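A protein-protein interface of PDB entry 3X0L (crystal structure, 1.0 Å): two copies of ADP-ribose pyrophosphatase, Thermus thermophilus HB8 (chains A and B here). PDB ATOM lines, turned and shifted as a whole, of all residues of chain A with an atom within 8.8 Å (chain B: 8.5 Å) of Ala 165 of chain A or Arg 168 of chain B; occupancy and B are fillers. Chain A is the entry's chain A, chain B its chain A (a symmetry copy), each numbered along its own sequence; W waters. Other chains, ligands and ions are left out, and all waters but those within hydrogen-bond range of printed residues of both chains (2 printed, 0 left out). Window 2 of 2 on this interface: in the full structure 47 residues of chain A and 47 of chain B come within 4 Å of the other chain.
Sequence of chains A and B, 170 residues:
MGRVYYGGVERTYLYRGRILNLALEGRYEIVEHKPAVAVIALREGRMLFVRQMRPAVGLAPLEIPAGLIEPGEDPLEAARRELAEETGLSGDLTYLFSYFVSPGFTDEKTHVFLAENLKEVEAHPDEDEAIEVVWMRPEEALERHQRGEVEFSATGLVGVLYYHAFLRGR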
ATOM      1  N   PHE A  97      -4.350  -7.381 -21.604  1.00  0.00           N
ATOM      2  CA  PHE A  97      -3.684  -7.051 -22.882  1.00  0.00           C
ATOM      3  C   PHE A  97      -4.380  -5.794 -23.407  1.00  0.00           C
ATOM      4  O   PHE A  97      -5.430  -5.364 -22.878  1.00  0.00           O
ATOM      5  CB  PHE A  97      -3.736  -8.197 -23.912  1.00  0.00           C
ATOM      6  CG  PHE A  97      -5.023  -8.989 -23.943  1.00  0.00           C
ATOM      7  CD1 PHE A  97      -4.959 -10.370 -23.660  1.00  0.00           C
ATOM      8  CD2 PHE A  97      -6.240  -8.400 -24.262  1.00  0.00           C
ATOM      9  CE1 PHE A  97      -6.126 -11.143 -23.657  1.00  0.00           C
ATOM     10  CE2 PHE A  97      -7.418  -9.154 -24.245  1.00  0.00           C
ATOM     11  CZ  PHE A  97      -7.350 -10.543 -23.945  1.00  0.00           C
ATOM     12  N   PRO A 138     -20.972 -17.320 -22.970  1.00  0.00           N
ATOM     13  CA  PRO A 138     -20.270 -16.944 -24.214  1.00  0.00           C
ATOM     14  C   PRO A 138     -20.543 -17.904 -25.373  1.00  0.00           C
ATOM     15  O   PRO A 138     -20.501 -17.476 -26.502  1.00  0.00           O
ATOM     16  CB  PRO A 138     -18.812 -16.998 -23.812  1.00  0.00           C
ATOM     17  CG  PRO A 138     -18.850 -16.688 -22.335  1.00  0.00           C
ATOM     18  CD  PRO A 138     -20.053 -17.426 -21.804  1.00  0.00           C
ATOM     19  N   VAL A 158     -13.744 -10.097 -28.343  1.00  0.00           N
ATOM     20  CA  VAL A 158     -12.540 -10.397 -27.538  1.00  0.00           C
ATOM     21  C   VAL A 158     -12.941 -11.088 -26.272  1.00  0.00           C
ATOM     22  O   VAL A 158     -12.290 -12.072 -25.861  1.00  0.00           O
ATOM     23  CB  VAL A 158     -11.750  -9.084 -27.281  1.00  0.00           C
ATOM     24  CG1 VAL A 158     -10.760  -9.264 -26.150  1.00  0.00           C
ATOM     25  CG2 VAL A 158     -11.068  -8.658 -28.577  1.00  0.00           C
ATOM     26  N   GLY A 159     -14.007 -10.649 -25.597  1.00  0.00           N
ATOM     27  CA  GLY A 159     -14.423 -11.334 -24.365  1.00  0.00           C
ATOM     28  C   GLY A 159     -14.794 -12.779 -24.647  1.00  0.00           C
ATOM     29  O   GLY A 159     -14.391 -13.693 -23.915  1.00  0.00           O
ATOM     30  N   VAL A 160     -15.575 -13.018 -25.695  1.00  0.00           N
ATOM     31  CA  VAL A 160     -15.992 -14.382 -26.012  1.00  0.00           C
ATOM     32  C   VAL A 160     -14.805 -15.261 -26.347  1.00  0.00           C
ATOM     33  O   VAL A 160     -14.719 -16.413 -25.896  1.00  0.00           O
ATOM     34  CB  VAL A 160     -16.987 -14.348 -27.193  1.00  0.00           C
ATOM     35  CG1 VAL A 160     -17.211 -15.704 -27.842  1.00  0.00           C
ATOM     36  CG2 VAL A 160     -18.335 -13.759 -26.734  1.00  0.00           C
ATOM     37  N   LEU A 161     -13.876 -14.745 -27.153  1.00  0.00           N
ATOM     38  CA  LEU A 161     -12.710 -15.566 -27.519  1.00  0.00           C
ATOM     39  C   LEU A 161     -11.792 -15.816 -26.347  1.00  0.00           C
ATOM     40  O   LEU A 161     -11.287 -16.931 -26.180  1.00  0.00           O
ATOM     41  CB  LEU A 161     -11.952 -14.948 -28.697  1.00  0.00           C
ATOM     42  CG  LEU A 161     -12.764 -14.822 -29.991  1.00  0.00           C
ATOM     43  CD1 LEU A 161     -11.936 -14.091 -31.058  1.00  0.00           C
ATOM     44  CD2 LEU A 161     -13.196 -16.200 -30.513  1.00  0.00           C
ATOM     45  N   TYR A 162     -11.561 -14.773 -25.515  1.00  0.00           N
ATOM     46  CA  TYR A 162     -10.719 -14.981 -24.349  1.00  0.00           C
ATOM     47  C   TYR A 162     -11.305 -16.046 -23.431  1.00  0.00           C
ATOM     48  O   TYR A 162     -10.585 -16.896 -22.904  1.00  0.00           O
ATOM     49  CB  TYR A 162     -10.615 -13.615 -23.598  1.00  0.00           C
ATOM     50  CG  TYR A 162      -9.715 -13.771 -22.374  1.00  0.00           C
ATOM     51  CD1 TYR A 162      -8.353 -13.712 -22.518  1.00  0.00           C
ATOM     52  CD2 TYR A 162     -10.244 -14.044 -21.124  1.00  0.00           C
ATOM     53  CE1 TYR A 162      -7.483 -13.879 -21.438  1.00  0.00           C
ATOM     54  CE2 TYR A 162      -9.403 -14.232 -20.032  1.00  0.00           C
ATOM     55  CZ  TYR A 162      -8.056 -14.129 -20.206  1.00  0.00           C
ATOM     56  OH  TYR A 162      -7.234 -14.338 -19.095  1.00  0.00           O
ATOM     57  N   TYR A 163     -12.625 -16.000 -23.203  1.00  0.00           N
ATOM     58  CA  TYR A 163     -13.265 -17.021 -22.382  1.00  0.00           C
ATOM     59  C   TYR A 163     -12.995 -18.396 -22.937  1.00  0.00           C
ATOM     60  O   TYR A 163     -12.654 -19.319 -22.221  1.00  0.00           O
ATOM     61  CB  TYR A 163     -14.794 -16.754 -22.303  1.00  0.00           C
ATOM     62  CG  TYR A 163     -15.567 -17.986 -21.876  1.00  0.00           C
ATOM     63  CD1 TYR A 163     -15.745 -18.285 -20.537  1.00  0.00           C
ATOM     64  CD2 TYR A 163     -16.152 -18.843 -22.828  1.00  0.00           C
ATOM     65  CE1 TYR A 163     -16.470 -19.440 -20.178  1.00  0.00           C
ATOM     66  CE2 TYR A 163     -16.852 -19.988 -22.500  1.00  0.00           C
ATOM     67  CZ  TYR A 163     -16.997 -20.240 -21.173  1.00  0.00           C
ATOM     68  OH  TYR A 163     -17.727 -21.399 -20.779  1.00  0.00           O
ATOM     69  N   HIS A 164     -13.232 -18.579 -24.256  1.00  0.00           N
ATOM     70  CA  HIS A 164     -13.084 -19.929 -24.809  1.00  0.00           C
ATOM     71  C   HIS A 164     -11.628 -20.386 -24.720  1.00  0.00           C
ATOM     72  O   HIS A 164     -11.372 -21.546 -24.515  1.00  0.00           O
ATOM     73  CB  HIS A 164     -13.584 -19.949 -26.246  1.00  0.00           C
ATOM     74  CG  HIS A 164     -15.014 -20.039 -26.417  1.00  0.00           C
ATOM     75  ND1 HIS A 164     -15.827 -18.909 -26.450  1.00  0.00           N
ATOM     76  CD2 HIS A 164     -15.835 -21.146 -26.583  1.00  0.00           C
ATOM     77  CE1 HIS A 164     -17.085 -19.329 -26.627  1.00  0.00           C
ATOM     78  NE2 HIS A 164     -17.138 -20.639 -26.728  1.00  0.00           N
ATOM     79  N   ALA A 165     -10.706 -19.454 -24.874  1.00  0.00           N
ATOM     80  CA  ALA A 165      -9.250 -19.790 -24.825  1.00  0.00           C
ATOM     81  C   ALA A 165      -8.809 -20.131 -23.422  1.00  0.00           C
ATOM     82  O   ALA A 165      -8.040 -21.091 -23.264  1.00  0.00           O
ATOM     83  CB  ALA A 165      -8.413 -18.627 -25.345  1.00  0.00           C
ATOM     84  N   PHE A 166      -9.254 -19.396 -22.400  1.00  0.00           N
ATOM     85  CA  PHE A 166      -8.592 -19.476 -21.111  1.00  0.00           C
ATOM     86  C   PHE A 166      -9.455 -19.681 -19.926  1.00  0.00           C
ATOM     87  O   PHE A 166      -8.869 -20.010 -18.843  1.00  0.00           O
ATOM     88  CB  PHE A 166      -7.788 -18.164 -20.869  1.00  0.00           C
ATOM     89  CG  PHE A 166      -6.727 -17.966 -21.963  1.00  0.00           C
ATOM     90  CD1 PHE A 166      -6.763 -16.888 -22.825  1.00  0.00           C
ATOM     91  CD2 PHE A 166      -5.664 -18.871 -22.109  1.00  0.00           C
ATOM     92  CE1 PHE A 166      -5.789 -16.715 -23.793  1.00  0.00           C
ATOM     93  CE2 PHE A 166      -4.713 -18.719 -23.133  1.00  0.00           C
ATOM     94  CZ  PHE A 166      -4.747 -17.622 -23.980  1.00  0.00           C
ATOM     95  N   LEU A 167     -10.772 -19.546 -20.020  1.00  0.00           N
ATOM     96  CA  LEU A 167     -11.615 -19.551 -18.797  1.00  0.00           C
ATOM     97  C   LEU A 167     -12.549 -20.718 -18.668  1.00  0.00           C
ATOM     98  O   LEU A 167     -13.382 -20.706 -17.739  1.00  0.00           O
ATOM     99  CB  LEU A 167     -12.407 -18.246 -18.774  1.00  0.00           C
ATOM    100  CG  LEU A 167     -11.640 -16.964 -18.733  1.00  0.00           C
ATOM    101  CD1 LEU A 167     -12.612 -15.753 -18.668  1.00  0.00           C
ATOM    102  CD2 LEU A 167     -10.671 -16.936 -17.520  1.00  0.00           C
ATOM    103  N   ARG A 168     -12.401 -21.723 -19.502  1.00  0.00           N
ATOM    104  CA  ARG A 168     -13.298 -22.876 -19.319  1.00  0.00           C
ATOM    105  C   ARG A 168     -12.725 -23.935 -18.341  1.00  0.00           C
ATOM    106  O   ARG A 168     -13.718 -24.596 -17.878  1.00  0.00           O
ATOM    107  CB  ARG A 168     -13.664 -23.520 -20.691  1.00  0.00           C
ATOM    108  CG  ARG A 168     -14.439 -22.513 -21.624  1.00  0.00           C
ATOM    109  CD  ARG A 168     -14.898 -23.241 -22.875  1.00  0.00           C
ATOM    110  NE  ARG A 168     -13.767 -23.432 -23.783  1.00  0.00           N
ATOM    111  CZ  ARG A 168     -13.766 -24.056 -24.960  1.00  0.00           C
ATOM    112  NH1 ARG A 168     -14.983 -24.583 -25.247  1.00  0.00           N
ATOM    113  NH2 ARG A 168     -12.656 -24.152 -25.694  1.00  0.00           N
ATOM    114  N   LEU B  42      -2.868 -20.466 -40.121  1.00  0.00           N
ATOM    115  CA  LEU B  42      -1.933 -21.219 -39.295  1.00  0.00           C
ATOM    116  C   LEU B  42      -1.219 -22.246 -40.157  1.00  0.00           C
ATOM    117  O   LEU B  42      -1.851 -22.922 -40.966  1.00  0.00           O
ATOM    118  CB  LEU B  42      -2.677 -21.921 -38.154  1.00  0.00           C
ATOM    119  CG  LEU B  42      -1.851 -22.449 -36.977  1.00  0.00           C
ATOM    120  CD1 LEU B  42      -1.428 -21.305 -36.065  1.00  0.00           C
ATOM    121  CD2 LEU B  42      -2.634 -23.494 -36.198  1.00  0.00           C
ATOM    122  N   GLY B  45       2.056 -24.578 -36.783  1.00  0.00           N
ATOM    123  CA  GLY B  45       2.014 -23.979 -35.444  1.00  0.00           C
ATOM    124  C   GLY B  45       2.261 -22.464 -35.441  1.00  0.00           C
ATOM    125  O   GLY B  45       2.183 -21.844 -34.372  1.00  0.00           O
ATOM    126  N   ARG B 137       4.558 -18.251 -33.782  1.00  0.00           N
ATOM    127  CA  ARG B 137       3.624 -18.966 -32.915  1.00  0.00           C
ATOM    128  C   ARG B 137       2.701 -18.016 -32.151  1.00  0.00           C
ATOM    129  O   ARG B 137       3.198 -17.045 -31.558  1.00  0.00           O
ATOM    130  CB  ARG B 137       4.352 -19.759 -31.798  1.00  0.00           C
ATOM    131  CG  ARG B 137       5.169 -20.939 -32.341  1.00  0.00           C
ATOM    132  CD  ARG B 137       5.791 -21.716 -31.185  1.00  0.00           C
ATOM    133  NE  ARG B 137       4.922 -22.359 -30.224  1.00  0.00           N
ATOM    134  CZ  ARG B 137       4.783 -22.242 -28.906  1.00  0.00           C
ATOM    135  NH1 ARG B 137       3.922 -22.939 -28.148  1.00  0.00           N
ATOM    136  NH2 ARG B 137       5.545 -21.357 -28.257  1.00  0.00           N
ATOM    137  N   PRO B 138       1.391 -18.214 -32.096  1.00  0.00           N
ATOM    138  CA  PRO B 138       0.544 -17.271 -31.336  1.00  0.00           C
ATOM    139  C   PRO B 138       0.913 -17.189 -29.854  1.00  0.00           C
ATOM    140  O   PRO B 138       0.712 -16.156 -29.263  1.00  0.00           O
ATOM    141  CB  PRO B 138      -0.844 -17.848 -31.506  1.00  0.00           C
ATOM    142  CG  PRO B 138      -0.763 -18.557 -32.836  1.00  0.00           C
ATOM    143  CD  PRO B 138       0.594 -19.216 -32.854  1.00  0.00           C
ATOM    144  N   GLU B 139       1.383 -18.289 -29.286  1.00  0.00           N
ATOM    145  CA  GLU B 139       1.818 -18.241 -27.863  1.00  0.00           C
ATOM    146  C   GLU B 139       2.914 -17.233 -27.690  1.00  0.00           C
ATOM    147  O   GLU B 139       3.032 -16.538 -26.710  1.00  0.00           O
ATOM    148  CB  GLU B 139       2.311 -19.648 -27.494  1.00  0.00           C
ATOM    149  CG  GLU B 139       1.193 -20.707 -27.510  1.00  0.00           C
ATOM    150  CD  GLU B 139       1.026 -21.459 -28.815  1.00  0.00           C
ATOM    151  OE1 GLU B 139       1.541 -20.977 -29.899  1.00  0.00           O
ATOM    152  OE2 GLU B 139       0.383 -22.519 -28.839  1.00  0.00           O
ATOM    153  N   LEU B 142       1.612 -13.590 -28.011  1.00  0.00           N
ATOM    154  CA  LEU B 142       0.982 -13.124 -26.748  1.00  0.00           C
ATOM    155  C   LEU B 142       2.034 -12.886 -25.698  1.00  0.00           C
ATOM    156  O   LEU B 142       1.932 -11.872 -25.005  1.00  0.00           O
ATOM    157  CB  LEU B 142      -0.040 -14.219 -26.319  1.00  0.00           C
ATOM    158  CG  LEU B 142      -0.807 -13.923 -25.024  1.00  0.00           C
ATOM    159  CD1 LEU B 142      -1.484 -12.563 -25.073  1.00  0.00           C
ATOM    160  CD2 LEU B 142      -1.751 -15.105 -24.825  1.00  0.00           C
ATOM    161  N   VAL B 160      -4.910 -14.306 -32.389  1.00  0.00           N
ATOM    162  CA  VAL B 160      -4.262 -15.035 -31.302  1.00  0.00           C
ATOM    163  C   VAL B 160      -5.279 -15.702 -30.399  1.00  0.00           C
ATOM    164  O   VAL B 160      -5.110 -16.864 -29.999  1.00  0.00           O
ATOM    165  CB  VAL B 160      -3.378 -14.063 -30.491  1.00  0.00           C
ATOM    166  CG1 VAL B 160      -2.944 -14.611 -29.142  1.00  0.00           C
ATOM    167  CG2 VAL B 160      -2.139 -13.661 -31.315  1.00  0.00           C
ATOM    168  N   LEU B 161      -6.344 -14.980 -30.048  1.00  0.00           N
ATOM    169  CA  LEU B 161      -7.354 -15.579 -29.160  1.00  0.00           C
ATOM    170  C   LEU B 161      -8.122 -16.693 -29.831  1.00  0.00           C
ATOM    171  O   LEU B 161      -8.390 -17.726 -29.207  1.00  0.00           O
ATOM    172  CB  LEU B 161      -8.297 -14.511 -28.602  1.00  0.00           C
ATOM    173  CG  LEU B 161      -7.619 -13.432 -27.751  1.00  0.00           C
ATOM    174  CD1 LEU B 161      -8.644 -12.364 -27.346  1.00  0.00           C
ATOM    175  CD2 LEU B 161      -6.967 -14.039 -26.499  1.00  0.00           C
ATOM    176  N   TYR B 162      -8.490 -16.495 -31.119  1.00  0.00           N
ATOM    177  CA  TYR B 162      -9.192 -17.559 -31.817  1.00  0.00           C
ATOM    178  C   TYR B 162      -8.349 -18.827 -31.877  1.00  0.00           C
ATOM    179  O   TYR B 162      -8.853 -19.934 -31.685  1.00  0.00           O
ATOM    180  CB  TYR B 162      -9.502 -17.045 -33.259  1.00  0.00           C
ATOM    181  CG  TYR B 162     -10.267 -18.119 -34.031  1.00  0.00           C
ATOM    182  CD1 TYR B 162     -11.622 -18.244 -33.863  1.00  0.00           C
ATOM    183  CD2 TYR B 162      -9.609 -19.021 -34.849  1.00  0.00           C
ATOM    184  CE1 TYR B 162     -12.366 -19.227 -34.520  1.00  0.00           C
ATOM    185  CE2 TYR B 162     -10.318 -20.022 -35.504  1.00  0.00           C
ATOM    186  CZ  TYR B 162     -11.670 -20.092 -35.342  1.00  0.00           C
ATOM    187  OH  TYR B 162     -12.356 -21.118 -35.999  1.00  0.00           O
ATOM    188  N   TYR B 163      -7.050 -18.685 -32.174  1.00  0.00           N
ATOM    189  CA  TYR B 163      -6.169 -19.847 -32.192  1.00  0.00           C
ATOM    190  C   TYR B 163      -6.209 -20.565 -30.868  1.00  0.00           C
ATOM    191  O   TYR B 163      -6.315 -21.776 -30.800  1.00  0.00           O
ATOM    192  CB  TYR B 163      -4.718 -19.406 -32.532  1.00  0.00           C
ATOM    193  CG  TYR B 163      -3.695 -20.447 -32.123  1.00  0.00           C
ATOM    194  CD1 TYR B 163      -3.368 -21.492 -32.967  1.00  0.00           C
ATOM    195  CD2 TYR B 163      -3.025 -20.361 -30.887  1.00  0.00           C
ATOM    196  CE1 TYR B 163      -2.412 -22.443 -32.552  1.00  0.00           C
ATOM    197  CE2 TYR B 163      -2.096 -21.288 -30.454  1.00  0.00           C
ATOM    198  CZ  TYR B 163      -1.812 -22.299 -31.316  1.00  0.00           C
ATOM    199  OH  TYR B 163      -0.848 -23.272 -30.926  1.00  0.00           O
ATOM    200  N   HIS B 164      -6.035 -19.810 -29.759  1.00  0.00           N
ATOM    201  CA  HIS B 164      -5.959 -20.487 -28.460  1.00  0.00           C
ATOM    202  C   HIS B 164      -7.291 -21.164 -28.133  1.00  0.00           C
ATOM    203  O   HIS B 164      -7.304 -22.206 -27.528  1.00  0.00           O
ATOM    204  CB  HIS B 164      -5.567 -19.486 -27.385  1.00  0.00           C
ATOM    205  CG  HIS B 164      -4.163 -19.167 -27.297  1.00  0.00           C
ATOM    206  ND1 HIS B 164      -3.586 -18.151 -28.054  1.00  0.00           N
ATOM    207  CD2 HIS B 164      -3.158 -19.727 -26.519  1.00  0.00           C
ATOM    208  CE1 HIS B 164      -2.286 -18.108 -27.738  1.00  0.00           C
ATOM    209  NE2 HIS B 164      -1.990 -19.007 -26.825  1.00  0.00           N
ATOM    210  N   ALA B 165      -8.383 -20.549 -28.547  1.00  0.00           N
ATOM    211  CA  ALA B 165      -9.740 -21.109 -28.267  1.00  0.00           C
ATOM    212  C   ALA B 165     -10.007 -22.347 -29.090  1.00  0.00           C
ATOM    213  O   ALA B 165     -10.565 -23.310 -28.541  1.00  0.00           O
ATOM    214  CB  ALA B 165     -10.819 -20.072 -28.556  1.00  0.00           C
ATOM    215  N   PHE B 166      -9.640 -22.371 -30.373  1.00  0.00           N
ATOM    216  CA  PHE B 166     -10.183 -23.383 -31.260  1.00  0.00           C
ATOM    217  C   PHE B 166      -9.215 -24.130 -32.095  1.00  0.00           C
ATOM    218  O   PHE B 166      -9.649 -25.181 -32.672  1.00  0.00           O
ATOM    219  CB  PHE B 166     -11.203 -22.718 -32.230  1.00  0.00           C
ATOM    220  CG  PHE B 166     -12.358 -22.073 -31.446  1.00  0.00           C
ATOM    221  CD1 PHE B 166     -12.590 -20.712 -31.480  1.00  0.00           C
ATOM    222  CD2 PHE B 166     -13.236 -22.856 -30.679  1.00  0.00           C
ATOM    223  CE1 PHE B 166     -13.645 -20.150 -30.782  1.00  0.00           C
ATOM    224  CE2 PHE B 166     -14.267 -22.269 -29.927  1.00  0.00           C
ATOM    225  CZ  PHE B 166     -14.504 -20.904 -29.985  1.00  0.00           C
ATOM    226  N   LEU B 167      -7.958 -23.716 -32.203  1.00  0.00           N
ATOM    227  CA  LEU B 167      -7.045 -24.341 -33.194  1.00  0.00           C
ATOM    228  C   LEU B 167      -5.898 -25.113 -32.610  1.00  0.00           C
ATOM    229  O   LEU B 167      -5.019 -25.539 -33.387  1.00  0.00           O
ATOM    230  CB  LEU B 167      -6.519 -23.234 -34.104  1.00  0.00           C
ATOM    231  CG  LEU B 167      -7.513 -22.456 -34.903  1.00  0.00           C
ATOM    232  CD1 LEU B 167      -6.788 -21.411 -35.797  1.00  0.00           C
ATOM    233  CD2 LEU B 167      -8.381 -23.398 -35.779  1.00  0.00           C
ATOM    234  N   ARG B 168      -5.909 -25.354 -31.318  1.00  0.00           N
ATOM    235  CA  ARG B 168      -4.796 -26.155 -30.783  1.00  0.00           C
ATOM    236  C   ARG B 168      -5.085 -27.680 -30.810  1.00  0.00           C
ATOM    237  O   ARG B 168      -3.953 -28.277 -30.810  1.00  0.00           O
ATOM    238  CB  ARG B 168      -4.412 -25.684 -29.347  1.00  0.00           C
ATOM    239  CG  ARG B 168      -3.912 -24.190 -29.334  1.00  0.00           C
ATOM    240  CD  ARG B 168      -3.411 -23.840 -27.943  1.00  0.00           C
ATOM    241  NE  ARG B 168      -4.546 -23.617 -27.047  1.00  0.00           N
ATOM    242  CZ  ARG B 168      -4.510 -23.326 -25.748  1.00  0.00           C
ATOM    243  NH1 ARG B 168      -3.238 -23.301 -25.277  1.00  0.00           N
ATOM    244  NH2 ARG B 168      -5.630 -23.141 -25.047  1.00  0.00           N
HETATM  245  O   HOH W   1     -12.499 -25.584 -28.122  1.00  0.00           O
HETATM  246  O   HOH W   2      -5.680 -22.678 -22.263  1.00  0.00           O
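ND1 of His 164 of chain B sits at hydrogen-bond distance from O of Val 160 of chain B, 2.8 Å away.
NE of Arg 168 of chain A is in hydrogen-bond range of O of His 164 of chain A.
The guanidinium group of Arg 168 of chain B is in hydrogen-bond range of the backbone carbonyl oxygen of His 164 of chain B (3.1 Å).
O of Val 160 of chain A sits at hydrogen-bond distance from ND1 of His 164 of chain A (2.8 Å).
Among the printed residues, pairs that only touch across the chains: Val 158 of chain A with Leu 161 of chain B (3.9 Å), Leu 161 of chain A with Leu 161 of chain B (3.7 Å), Leu 161 of chain A with Ala 165 of chain B (3.97 Å), Leu 161 of chain A with Phe 166 of chain B (3.98 Å), His 164 of chain A with Ala 165 of chain B (3.6 Å), His 164 of chain A with Phe 166 of chain B (3.7 Å), Ala 165 of chain A with Leu 161 of chain B (3.97 Å), Ala 165 of chain A with His 164 of chain B (3.6 Å), Ala 165 of chain A with Ala 165 of chain B (3.7 Å), Ala 165 of chain A with Arg 168 of chain B (3.6 Å), Phe 166 of chain A with Leu 161 of chain B (3.98 Å), Phe 166 of chain A with His 164 of chain B (3.7 Å) and Arg 168 of chain A with Ala 165 of chain B (3.6 Å).
Of the printed residues of chain B, Val 158 of chain A touches Leu 161 (3.9 Å).
Ala 165 of chain A touches just these residues of chain B: Leu 161, His 164, Ala 165 and Arg 168.
Printed residues of chain B within 4 Å of Phe 166 of chain A: Leu 161 (3.98 Å) and His 164 (3.7 Å).
Of the printed residues of chain B, Arg 168 of chain A touches Ala 165.
Leu 142 of chain B touches none of the printed residues of chain A.
Of the printed residues of chain A, His 164 of chain B touches Ala 165 and Phe 166.
Arg 168 of chain B touches just one residue of chain A: Ala 165.
Among the printed residues, 13 pairs touch across the chains.
Among the printed residues, no Asp or Glu carboxylate lies within 4 Å of a Lys or Arg side-chain nitrogen of the other chain.
Leu 161 of chain A touches its own counterpart, Leu 161 of chain B.
Leu 161 of chain A touches Ala 165 of chain B, and with the chains exchanged Ala 165 of chain A touches Leu 161 of chain B.
Leu 161 of chain A touches Phe 166 of chain B, and with the chains exchanged Phe 166 of chain A touches Leu 161 of chain B.
Ala 165 of chain B touches its own counterpart, Ala 165 of chain A.
Positions printed for both chains: 138, 160, 161, 162, 163, 164, 165, 166, 167 and 168.
Of the 13 pairs that touch across the chains among the printed residues, 12 have their exchanged pair printed and touching as well.
Water W1 lies within hydrogen-bond range of the guanidinium group (NH2) of Arg 168 of chain A (2.8 Å) and the backbone carbonyl oxygen (O) of Ala 165 of chain B (3.0 Å).
Water W2 bridges the guanidinium group (NH2) of Arg 168 of chain B (2.8 Å) and the backbone carbonyl oxygen (O) of Ala 165 of chain A (3.0 Å).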
